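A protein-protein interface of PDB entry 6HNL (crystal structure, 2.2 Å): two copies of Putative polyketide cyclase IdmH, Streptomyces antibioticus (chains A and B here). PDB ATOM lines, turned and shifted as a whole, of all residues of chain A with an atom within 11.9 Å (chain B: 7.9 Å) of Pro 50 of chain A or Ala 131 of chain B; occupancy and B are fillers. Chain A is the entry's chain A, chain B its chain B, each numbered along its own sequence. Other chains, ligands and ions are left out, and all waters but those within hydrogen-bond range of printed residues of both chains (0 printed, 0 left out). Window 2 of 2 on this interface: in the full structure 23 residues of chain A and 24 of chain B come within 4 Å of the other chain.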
ATOM      1  N   ILE A  37      -9.624   0.239   5.744  1.00  0.00           N
ATOM      2  CA  ILE A  37     -10.014  -1.146   6.005  1.00  0.00           C
ATOM      3  C   ILE A  37     -11.507  -1.331   5.730  1.00  0.00           C
ATOM      4  O   ILE A  37     -12.344  -0.809   6.461  1.00  0.00           O
ATOM      5  CB  ILE A  37      -9.718  -1.560   7.459  1.00  0.00           C
ATOM      6  CG1 ILE A  37      -8.278  -1.189   7.884  1.00  0.00           C
ATOM      7  CG2 ILE A  37      -9.969  -3.050   7.637  1.00  0.00           C
ATOM      8  CD1 ILE A  37      -7.181  -1.809   7.043  1.00  0.00           C
ATOM      9  N   HIS A  38     -11.827  -2.097   4.698  1.00  0.00           N
ATOM     10  CA  HIS A  38     -13.202  -2.366   4.315  1.00  0.00           C
ATOM     11  C   HIS A  38     -13.639  -3.691   4.935  1.00  0.00           C
ATOM     12  O   HIS A  38     -13.286  -4.768   4.461  1.00  0.00           O
ATOM     13  CB  HIS A  38     -13.310  -2.448   2.800  1.00  0.00           C
ATOM     14  CG  HIS A  38     -12.817  -1.234   2.086  1.00  0.00           C
ATOM     15  ND1 HIS A  38     -13.603  -0.122   1.891  1.00  0.00           N
ATOM     16  CD2 HIS A  38     -11.630  -0.967   1.500  1.00  0.00           C
ATOM     17  CE1 HIS A  38     -12.920   0.789   1.220  1.00  0.00           C
ATOM     18  NE2 HIS A  38     -11.721   0.296   0.961  1.00  0.00           N
ATOM     19  N   LEU A  39     -14.370  -3.593   6.036  1.00  0.00           N
ATOM     20  CA  LEU A  39     -14.877  -4.737   6.739  1.00  0.00           C
ATOM     21  C   LEU A  39     -16.291  -5.016   6.241  1.00  0.00           C
ATOM     22  O   LEU A  39     -16.943  -4.122   5.701  1.00  0.00           O
ATOM     23  CB  LEU A  39     -14.884  -4.461   8.232  1.00  0.00           C
ATOM     24  CG  LEU A  39     -13.514  -4.275   8.875  1.00  0.00           C
ATOM     25  CD1 LEU A  39     -13.661  -3.966  10.355  1.00  0.00           C
ATOM     26  CD2 LEU A  39     -12.635  -5.505   8.655  1.00  0.00           C
ATOM     27  N   PRO A  40     -16.758  -6.267   6.396  1.00  0.00           N
ATOM     28  CA  PRO A  40     -18.110  -6.587   5.967  1.00  0.00           C
ATOM     29  C   PRO A  40     -19.168  -6.015   6.902  1.00  0.00           C
ATOM     30  O   PRO A  40     -18.862  -5.659   8.044  1.00  0.00           O
ATOM     31  CB  PRO A  40     -18.129  -8.120   5.972  1.00  0.00           C
ATOM     32  CG  PRO A  40     -17.075  -8.526   6.931  1.00  0.00           C
ATOM     33  CD  PRO A  40     -16.085  -7.408   7.049  1.00  0.00           C
ATOM     34  N   GLY A  41     -20.409  -5.967   6.423  1.00  0.00           N
ATOM     35  CA  GLY A  41     -21.541  -5.430   7.186  1.00  0.00           C
ATOM     36  C   GLY A  41     -21.768  -6.067   8.549  1.00  0.00           C
ATOM     37  O   GLY A  41     -22.261  -5.394   9.450  1.00  0.00           O
ATOM     38  N   THR A  42     -21.388  -7.340   8.712  1.00  0.00           N
ATOM     39  CA  THR A  42     -21.450  -8.016  10.020  1.00  0.00           C
ATOM     40  C   THR A  42     -20.630  -7.296  11.112  1.00  0.00           C
ATOM     41  O   THR A  42     -20.999  -7.327  12.287  1.00  0.00           O
ATOM     42  CB  THR A  42     -20.978  -9.492   9.950  1.00  0.00           C
ATOM     43  OG1 THR A  42     -19.637  -9.569   9.442  1.00  0.00           O
ATOM     44  CG2 THR A  42     -21.893 -10.346   9.069  1.00  0.00           C
ATOM     45  N   ALA A  43     -19.526  -6.653  10.713  1.00  0.00           N
ATOM     46  CA  ALA A  43     -18.704  -5.834  11.616  1.00  0.00           C
ATOM     47  C   ALA A  43     -19.243  -4.405  11.815  1.00  0.00           C
ATOM     48  O   ALA A  43     -18.650  -3.608  12.543  1.00  0.00           O
ATOM     49  CB  ALA A  43     -17.278  -5.777  11.096  1.00  0.00           C
ATOM     50  N   GLY A  44     -20.344  -4.065  11.148  1.00  0.00           N
ATOM     51  CA  GLY A  44     -21.036  -2.808  11.348  1.00  0.00           C
ATOM     52  C   GLY A  44     -21.636  -2.716  12.740  1.00  0.00           C
ATOM     53  O   GLY A  44     -21.832  -3.700  13.462  1.00  0.00           O
ATOM     54  N   ASP A  45     -21.996  -1.496  13.089  1.00  0.00           N
ATOM     55  CA  ASP A  45     -22.241  -1.100  14.481  1.00  0.00           C
ATOM     56  C   ASP A  45     -23.174   0.098  14.491  1.00  0.00           C
ATOM     57  O   ASP A  45     -23.359   0.745  13.452  1.00  0.00           O
ATOM     58  CB  ASP A  45     -20.875  -0.681  15.024  1.00  0.00           C
ATOM     59  CG  ASP A  45     -20.832  -0.518  16.500  1.00  0.00           C
ATOM     60  OD1 ASP A  45     -21.292  -1.439  17.202  1.00  0.00           O
ATOM     61  OD2 ASP A  45     -20.242   0.486  16.992  1.00  0.00           O
ATOM     62  N   ALA A  46     -23.680   0.466  15.665  1.00  0.00           N
ATOM     63  CA  ALA A  46     -24.487   1.688  15.830  1.00  0.00           C
ATOM     64  C   ALA A  46     -23.732   2.967  15.420  1.00  0.00           C
ATOM     65  O   ALA A  46     -24.301   3.836  14.768  1.00  0.00           O
ATOM     66  CB  ALA A  46     -24.979   1.799  17.267  1.00  0.00           C
ATOM     67  N   GLU A  47     -22.453   3.052  15.794  1.00  0.00           N
ATOM     68  CA  GLU A  47     -21.596   4.188  15.457  1.00  0.00           C
ATOM     69  C   GLU A  47     -20.921   4.095  14.070  1.00  0.00           C
ATOM     70  O   GLU A  47     -20.590   5.117  13.485  1.00  0.00           O
ATOM     71  CB  GLU A  47     -20.539   4.370  16.556  1.00  0.00           C
ATOM     72  CG  GLU A  47     -21.123   4.711  17.924  1.00  0.00           C
ATOM     73  CD  GLU A  47     -20.105   4.708  19.054  1.00  0.00           C
ATOM     74  OE1 GLU A  47     -18.910   5.029  18.839  1.00  0.00           O
ATOM     75  OE2 GLU A  47     -20.515   4.395  20.193  1.00  0.00           O
ATOM     76  N   HIS A  48     -20.705   2.886  13.570  1.00  0.00           N
ATOM     77  CA  HIS A  48     -20.053   2.651  12.268  1.00  0.00           C
ATOM     78  C   HIS A  48     -20.975   1.834  11.345  1.00  0.00           C
ATOM     79  O   HIS A  48     -20.926   0.604  11.387  1.00  0.00           O
ATOM     80  CB  HIS A  48     -18.705   1.932  12.420  1.00  0.00           C
ATOM     81  CG  HIS A  48     -17.678   2.716  13.174  1.00  0.00           C
ATOM     82  ND1 HIS A  48     -17.589   2.668  14.548  1.00  0.00           N
ATOM     83  CD2 HIS A  48     -16.704   3.561  12.762  1.00  0.00           C
ATOM     84  CE1 HIS A  48     -16.597   3.443  14.952  1.00  0.00           C
ATOM     85  NE2 HIS A  48     -16.046   4.000  13.887  1.00  0.00           N
ATOM     86  N   PRO A  49     -21.799   2.516  10.522  1.00  0.00           N
ATOM     87  CA  PRO A  49     -22.761   1.777   9.683  1.00  0.00           C
ATOM     88  C   PRO A  49     -22.087   0.868   8.648  1.00  0.00           C
ATOM     89  O   PRO A  49     -20.962   1.164   8.232  1.00  0.00           O
ATOM     90  CB  PRO A  49     -23.591   2.875   9.003  1.00  0.00           C
ATOM     91  CG  PRO A  49     -22.813   4.142   9.182  1.00  0.00           C
ATOM     92  CD  PRO A  49     -21.954   3.981  10.406  1.00  0.00           C
ATOM     93  N   PRO A  50     -22.771  -0.222   8.227  1.00  0.00           N
ATOM     94  CA  PRO A  50     -22.236  -1.141   7.207  1.00  0.00           C
ATOM     95  C   PRO A  50     -21.763  -0.431   5.913  1.00  0.00           C
ATOM     96  O   PRO A  50     -22.347   0.577   5.471  1.00  0.00           O
ATOM     97  CB  PRO A  50     -23.401  -2.091   6.942  1.00  0.00           C
ATOM     98  CG  PRO A  50     -24.191  -2.090   8.212  1.00  0.00           C
ATOM     99  CD  PRO A  50     -24.043  -0.712   8.802  1.00  0.00           C
ATOM    100  N   GLY A  51     -20.648  -0.897   5.377  1.00  0.00           N
ATOM    101  CA  GLY A  51     -20.027  -0.230   4.226  1.00  0.00           C
ATOM    102  C   GLY A  51     -19.218   1.020   4.517  1.00  0.00           C
ATOM    103  O   GLY A  51     -18.606   1.559   3.591  1.00  0.00           O
ATOM    104  N   THR A  52     -19.122   1.452   5.780  1.00  0.00           N
ATOM    105  CA  THR A  52     -18.194   2.532   6.168  1.00  0.00           C
ATOM    106  C   THR A  52     -16.797   1.939   6.403  1.00  0.00           C
ATOM    107  O   THR A  52     -16.671   1.024   7.207  1.00  0.00           O
ATOM    108  CB  THR A  52     -18.661   3.232   7.463  1.00  0.00           C
ATOM    109  OG1 THR A  52     -20.040   3.574   7.347  1.00  0.00           O
ATOM    110  CG2 THR A  52     -17.867   4.502   7.731  1.00  0.00           C
ATOM    111  N   PRO A  53     -15.755   2.443   5.709  1.00  0.00           N
ATOM    112  CA  PRO A  53     -14.379   1.975   5.978  1.00  0.00           C
ATOM    113  C   PRO A  53     -13.893   2.338   7.374  1.00  0.00           C
ATOM    114  O   PRO A  53     -14.324   3.332   7.946  1.00  0.00           O
ATOM    115  CB  PRO A  53     -13.514   2.730   4.950  1.00  0.00           C
ATOM    116  CG  PRO A  53     -14.461   3.279   3.948  1.00  0.00           C
ATOM    117  CD  PRO A  53     -15.793   3.435   4.619  1.00  0.00           C
ATOM    118  N   ARG A  54     -13.018   1.515   7.923  1.00  0.00           N
ATOM    119  CA  ARG A  54     -12.392   1.811   9.202  1.00  0.00           C
ATOM    120  C   ARG A  54     -10.921   2.145   8.955  1.00  0.00           C
ATOM    121  O   ARG A  54     -10.408   1.942   7.859  1.00  0.00           O
ATOM    122  CB  ARG A  54     -12.537   0.622  10.146  1.00  0.00           C
ATOM    123  CG  ARG A  54     -13.967   0.190  10.439  1.00  0.00           C
ATOM    124  CD  ARG A  54     -14.796   1.243  11.148  1.00  0.00           C
ATOM    125  NE  ARG A  54     -14.449   1.383  12.569  1.00  0.00           N
ATOM    126  CZ  ARG A  54     -14.823   0.536  13.539  1.00  0.00           C
ATOM    127  NH1 ARG A  54     -15.544  -0.564  13.275  1.00  0.00           N
ATOM    128  NH2 ARG A  54     -14.462   0.786  14.792  1.00  0.00           N
ATOM    129  N   VAL A  62     -12.274  -4.404  16.318  1.00  0.00           N
ATOM    130  CA  VAL A  62     -13.198  -5.460  15.899  1.00  0.00           C
ATOM    131  C   VAL A  62     -12.537  -6.843  16.032  1.00  0.00           C
ATOM    132  O   VAL A  62     -13.165  -7.823  16.461  1.00  0.00           O
ATOM    133  CB  VAL A  62     -13.671  -5.229  14.447  1.00  0.00           C
ATOM    134  CG1 VAL A  62     -14.396  -6.446  13.877  1.00  0.00           C
ATOM    135  CG2 VAL A  62     -14.561  -3.998  14.378  1.00  0.00           C
ATOM    136  N   TRP A 121      -9.555  -5.388   2.114  1.00  0.00           N
ATOM    137  CA  TRP A 121     -10.928  -5.852   2.040  1.00  0.00           C
ATOM    138  C   TRP A 121     -10.941  -7.271   2.596  1.00  0.00           C
ATOM    139  O   TRP A 121     -10.038  -8.058   2.274  1.00  0.00           O
ATOM    140  CB  TRP A 121     -11.416  -5.900   0.599  1.00  0.00           C
ATOM    141  CG  TRP A 121     -11.489  -4.582  -0.120  1.00  0.00           C
ATOM    142  CD1 TRP A 121     -12.604  -3.797  -0.285  1.00  0.00           C
ATOM    143  CD2 TRP A 121     -10.423  -3.911  -0.798  1.00  0.00           C
ATOM    144  NE1 TRP A 121     -12.284  -2.679  -1.016  1.00  0.00           N
ATOM    145  CE2 TRP A 121     -10.954  -2.725  -1.341  1.00  0.00           C
ATOM    146  CE3 TRP A 121      -9.066  -4.196  -0.992  1.00  0.00           C
ATOM    147  CZ2 TRP A 121     -10.179  -1.815  -2.063  1.00  0.00           C
ATOM    148  CZ3 TRP A 121      -8.285  -3.292  -1.716  1.00  0.00           C
ATOM    149  CH2 TRP A 121      -8.847  -2.110  -2.242  1.00  0.00           C
ATOM    150  N   THR A 122     -11.937  -7.598   3.418  1.00  0.00           N
ATOM    151  CA  THR A 122     -12.102  -8.969   3.929  1.00  0.00           C
ATOM    152  C   THR A 122     -13.587  -9.330   4.053  1.00  0.00           C
ATOM    153  O   THR A 122     -14.416  -8.467   4.347  1.00  0.00           O
ATOM    154  CB  THR A 122     -11.359  -9.198   5.261  1.00  0.00           C
ATOM    155  OG1 THR A 122     -11.474 -10.575   5.666  1.00  0.00           O
ATOM    156  CG2 THR A 122     -11.888  -8.312   6.374  1.00  0.00           C
ATOM    157  N   ILE A 123     -13.915 -10.587   3.775  1.00  0.00           N
ATOM    158  CA  ILE A 123     -15.246 -11.126   4.043  1.00  0.00           C
ATOM    159  C   ILE A 123     -15.067 -12.571   4.506  1.00  0.00           C
ATOM    160  O   ILE A 123     -14.252 -13.316   3.946  1.00  0.00           O
ATOM    161  CB  ILE A 123     -16.191 -11.109   2.811  1.00  0.00           C
ATOM    162  CG1 ILE A 123     -16.187  -9.743   2.108  1.00  0.00           C
ATOM    163  CG2 ILE A 123     -17.617 -11.432   3.245  1.00  0.00           C
ATOM    164  CD1 ILE A 123     -17.095  -9.646   0.897  1.00  0.00           C
ATOM    165  N   PHE B 102     -28.300  -0.429  -4.700  1.00  0.00           N
ATOM    166  CA  PHE B 102     -27.321  -1.030  -3.779  1.00  0.00           C
ATOM    167  C   PHE B 102     -25.963  -1.339  -4.447  1.00  0.00           C
ATOM    168  O   PHE B 102     -25.906  -1.566  -5.664  1.00  0.00           O
ATOM    169  CB  PHE B 102     -27.913  -2.286  -3.156  1.00  0.00           C
ATOM    170  CG  PHE B 102     -28.141  -3.417  -4.128  1.00  0.00           C
ATOM    171  CD1 PHE B 102     -27.113  -4.321  -4.447  1.00  0.00           C
ATOM    172  CD2 PHE B 102     -29.381  -3.608  -4.692  1.00  0.00           C
ATOM    173  CE1 PHE B 102     -27.326  -5.354  -5.334  1.00  0.00           C
ATOM    174  CE2 PHE B 102     -29.606  -4.658  -5.581  1.00  0.00           C
ATOM    175  CZ  PHE B 102     -28.575  -5.529  -5.900  1.00  0.00           C
ATOM    176  N   GLU B 103     -24.900  -1.334  -3.624  1.00  0.00           N
ATOM    177  CA  GLU B 103     -23.539  -1.689  -4.019  1.00  0.00           C
ATOM    178  C   GLU B 103     -22.971  -2.664  -2.984  1.00  0.00           C
ATOM    179  O   GLU B 103     -22.835  -2.319  -1.825  1.00  0.00           O
ATOM    180  CB  GLU B 103     -22.663  -0.444  -4.005  1.00  0.00           C
ATOM    181  CG  GLU B 103     -22.537   0.318  -5.313  1.00  0.00           C
ATOM    182  CD  GLU B 103     -21.369   1.301  -5.280  1.00  0.00           C
ATOM    183  OE1 GLU B 103     -21.093   1.892  -4.207  1.00  0.00           O
ATOM    184  OE2 GLU B 103     -20.713   1.496  -6.330  1.00  0.00           O
ATOM    185  N   ASP B 125     -20.810  -9.619   0.468  1.00  0.00           N
ATOM    186  CA  ASP B 125     -21.106  -8.822   1.647  1.00  0.00           C
ATOM    187  C   ASP B 125     -22.630  -8.553   1.754  1.00  0.00           C
ATOM    188  O   ASP B 125     -23.090  -7.420   1.585  1.00  0.00           O
ATOM    189  CB  ASP B 125     -20.300  -7.523   1.571  1.00  0.00           C
ATOM    190  CG  ASP B 125     -20.269  -6.761   2.890  1.00  0.00           C
ATOM    191  OD1 ASP B 125     -20.767  -7.261   3.920  1.00  0.00           O
ATOM    192  OD2 ASP B 125     -19.734  -5.634   2.901  1.00  0.00           O
ATOM    193  N   ASN B 126     -23.386  -9.604   2.054  1.00  0.00           N
ATOM    194  CA  ASN B 126     -24.858  -9.543   2.108  1.00  0.00           C
ATOM    195  C   ASN B 126     -25.412  -8.578   3.158  1.00  0.00           C
ATOM    196  O   ASN B 126     -26.417  -7.907   2.911  1.00  0.00           O
ATOM    197  CB  ASN B 126     -25.465 -10.936   2.315  1.00  0.00           C
ATOM    198  CG  ASN B 126     -25.130 -11.896   1.173  1.00  0.00           C
ATOM    199  OD1 ASN B 126     -24.576 -12.977   1.398  1.00  0.00           O
ATOM    200  ND2 ASN B 126     -25.436 -11.495  -0.057  1.00  0.00           N
ATOM    201  N   VAL B 127     -24.756  -8.494   4.313  1.00  0.00           N
ATOM    202  CA  VAL B 127     -25.229  -7.632   5.407  1.00  0.00           C
ATOM    203  C   VAL B 127     -25.149  -6.146   5.025  1.00  0.00           C
ATOM    204  O   VAL B 127     -26.063  -5.379   5.339  1.00  0.00           O
ATOM    205  CB  VAL B 127     -24.486  -7.918   6.734  1.00  0.00           C
ATOM    206  CG1 VAL B 127     -24.950  -6.967   7.841  1.00  0.00           C
ATOM    207  CG2 VAL B 127     -24.701  -9.376   7.151  1.00  0.00           C
ATOM    208  N   THR B 128     -24.079  -5.752   4.336  1.00  0.00           N
ATOM    209  CA  THR B 128     -23.943  -4.375   3.827  1.00  0.00           C
ATOM    210  C   THR B 128     -25.048  -4.038   2.818  1.00  0.00           C
ATOM    211  O   THR B 128     -25.594  -2.923   2.838  1.00  0.00           O
ATOM    212  CB  THR B 128     -22.549  -4.129   3.201  1.00  0.00           C
ATOM    213  OG1 THR B 128     -21.555  -4.209   4.231  1.00  0.00           O
ATOM    214  CG2 THR B 128     -22.445  -2.742   2.499  1.00  0.00           C
ATOM    215  N   MET B 129     -25.383  -4.997   1.955  1.00  0.00           N
ATOM    216  CA  MET B 129     -26.463  -4.822   0.968  1.00  0.00           C
ATOM    217  C   MET B 129     -27.812  -4.687   1.625  1.00  0.00           C
ATOM    218  O   MET B 129     -28.599  -3.839   1.219  1.00  0.00           O
ATOM    219  CB  MET B 129     -26.512  -6.008   0.014  1.00  0.00           C
ATOM    220  CG  MET B 129     -27.386  -5.755  -1.196  1.00  0.00           C
ATOM    221  SD  MET B 129     -27.704  -7.423  -2.184  1.00  0.00           S
ATOM    222  CE  MET B 129     -28.864  -8.269  -0.830  1.00  0.00           C
ATOM    223  N   LEU B 130     -28.092  -5.536   2.617  1.00  0.00           N
ATOM    224  CA  LEU B 130     -29.346  -5.467   3.370  1.00  0.00           C
ATOM    225  C   LEU B 130     -29.499  -4.122   4.093  1.00  0.00           C
ATOM    226  O   LEU B 130     -30.596  -3.560   4.119  1.00  0.00           O
ATOM    227  CB  LEU B 130     -29.468  -6.622   4.381  1.00  0.00           C
ATOM    228  CG  LEU B 130     -29.585  -8.085   3.898  1.00  0.00           C
ATOM    229  CD1 LEU B 130     -30.264  -8.943   4.960  1.00  0.00           C
ATOM    230  CD2 LEU B 130     -30.312  -8.231   2.566  1.00  0.00           C
ATOM    231  N   ALA B 131     -28.402  -3.607   4.651  1.00  0.00           N
ATOM    232  CA  ALA B 131     -28.408  -2.312   5.337  1.00  0.00           C
ATOM    233  C   ALA B 131     -28.827  -1.155   4.420  1.00  0.00           C
ATOM    234  O   ALA B 131     -29.579  -0.271   4.844  1.00  0.00           O
ATOM    235  CB  ALA B 131     -27.043  -2.035   5.944  1.00  0.00           C
ATOM    236  N   GLN B 132     -28.348  -1.178   3.174  1.00  0.00           N
ATOM    237  CA  GLN B 132     -28.692  -0.156   2.168  1.00  0.00           C
ATOM    238  C   GLN B 132     -30.166  -0.198   1.715  1.00  0.00           C
ATOM    239  O   GLN B 132     -30.720   0.837   1.346  1.00  0.00           O
ATOM    240  CB  GLN B 132     -27.785  -0.287   0.936  1.00  0.00           C
ATOM    241  CG  GLN B 132     -26.321   0.029   1.184  1.00  0.00           C
ATOM    242  CD  GLN B 132     -25.391  -0.513   0.101  1.00  0.00           C
ATOM    243  OE1 GLN B 132     -25.819  -1.173  -0.864  1.00  0.00           O
ATOM    244  NE2 GLN B 132     -24.095  -0.228   0.258  1.00  0.00           N
ATOM    245  N   LEU B 133     -30.772  -1.387   1.730  1.00  0.00           N
ATOM    246  CA  LEU B 133     -32.181  -1.567   1.354  1.00  0.00           C
ATOM    247  C   LEU B 133     -33.140  -1.502   2.556  1.00  0.00           C
ATOM    248  O   LEU B 133     -33.966  -0.585   2.654  1.00  0.00           O
ATOM    249  CB  LEU B 133     -32.376  -2.904   0.635  1.00  0.00           C
ATOM    250  CG  LEU B 133     -31.553  -3.154  -0.634  1.00  0.00           C
ATOM    251  CD1 LEU B 133     -31.899  -4.527  -1.193  1.00  0.00           C
ATOM    252  CD2 LEU B 133     -31.718  -2.075  -1.697  1.00  0.00           C
ATOM    253  N   GLY B 134     -33.043  -2.488   3.451  1.00  0.00           N
ATOM    254  CA  GLY B 134     -34.016  -2.692   4.530  1.00  0.00           C
ATOM    255  C   GLY B 134     -34.299  -4.171   4.733  1.00  0.00           C
ATOM    256  O   GLY B 134     -34.679  -4.877   3.795  1.00  0.00           O
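The backbone NH (N) of Gly 41 of chain A sits at hydrogen-bond distance from the side-chain carboxylate (OD1) of Asp 125 of chain B, 2.8 Å away. OG1 of Thr 128 of chain B lies within hydrogen-bond range of N of Gly 41 of chain A (3.0 Å).
Printed residues of chain B within 4 Å of Gly 41 of chain A: Asp 125, Val 127 and Thr 128. Of the printed residues of chain B, Thr 42 of chain A touches Val 127 (3.5 Å). Pro 50 of chain A touches two residues of chain B. Printed residues of chain B within 4 Å of Gly 51 of chain A: Thr 128 (3.6 Å). Of the printed residues of chain A, Asp 125 of chain B touches Pro 40 (3.4 Å), Gly 41 (2.8 Å) and Ile 123 (3.7 Å). Val 127 of chain B touches two residues of chain A. Ala 131 of chain B touches just one residue of chain A: Pro 50. No residue of chain A comes within 4 Å of Gln 132 of chain B. No residue of chain A comes within 4 Å of Leu 133 of chain B. Gly 134 of chain B touches none of the printed residues of chain A. The nearest residue of chain B that does not touch Pro 50 of chain A is Val 127 of chain B (4.5 Å). The nearest printed residue of chain A that does not touch Thr 128 of chain B is Pro 40 of chain A (4.01 Å).
No position is printed for both chains.
Among the printed residues, pairs that only touch across the chains: Pro 40 of chain A with Asp 125 of chain B (3.4 Å), Gly 41 of chain A with Val 127 of chain B (3.4 Å), Thr 42 of chain A with Val 127 of chain B (3.5 Å), Pro 50 of chain A with Thr 128 of chain B (3.9 Å), Pro 50 of chain A with Ala 131 of chain B (3.6 Å), Gly 51 of chain A with Thr 128 of chain B (3.6 Å) and Ile 123 of chain A with Asp 125 of chain B (3.7 Å).
Hydrophobic or aromatic side chains of chain A that line the printed part of chain B: Pro 40, Pro 50 and Ile 123. Along chain A the printed residues that touch a printed residue of chain B span positions 40 to 123. Among the printed residues, 9 pairs touch across the chains. Among the printed residues, no Asp or Glu carboxylate lies within 4 Å of a Lys or Arg side-chain nitrogen of the other chain.
OG1 of Thr 128 of chain B lies within hydrogen-bond range of OD2 of Asp 125 of chain B (2.7 Å).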
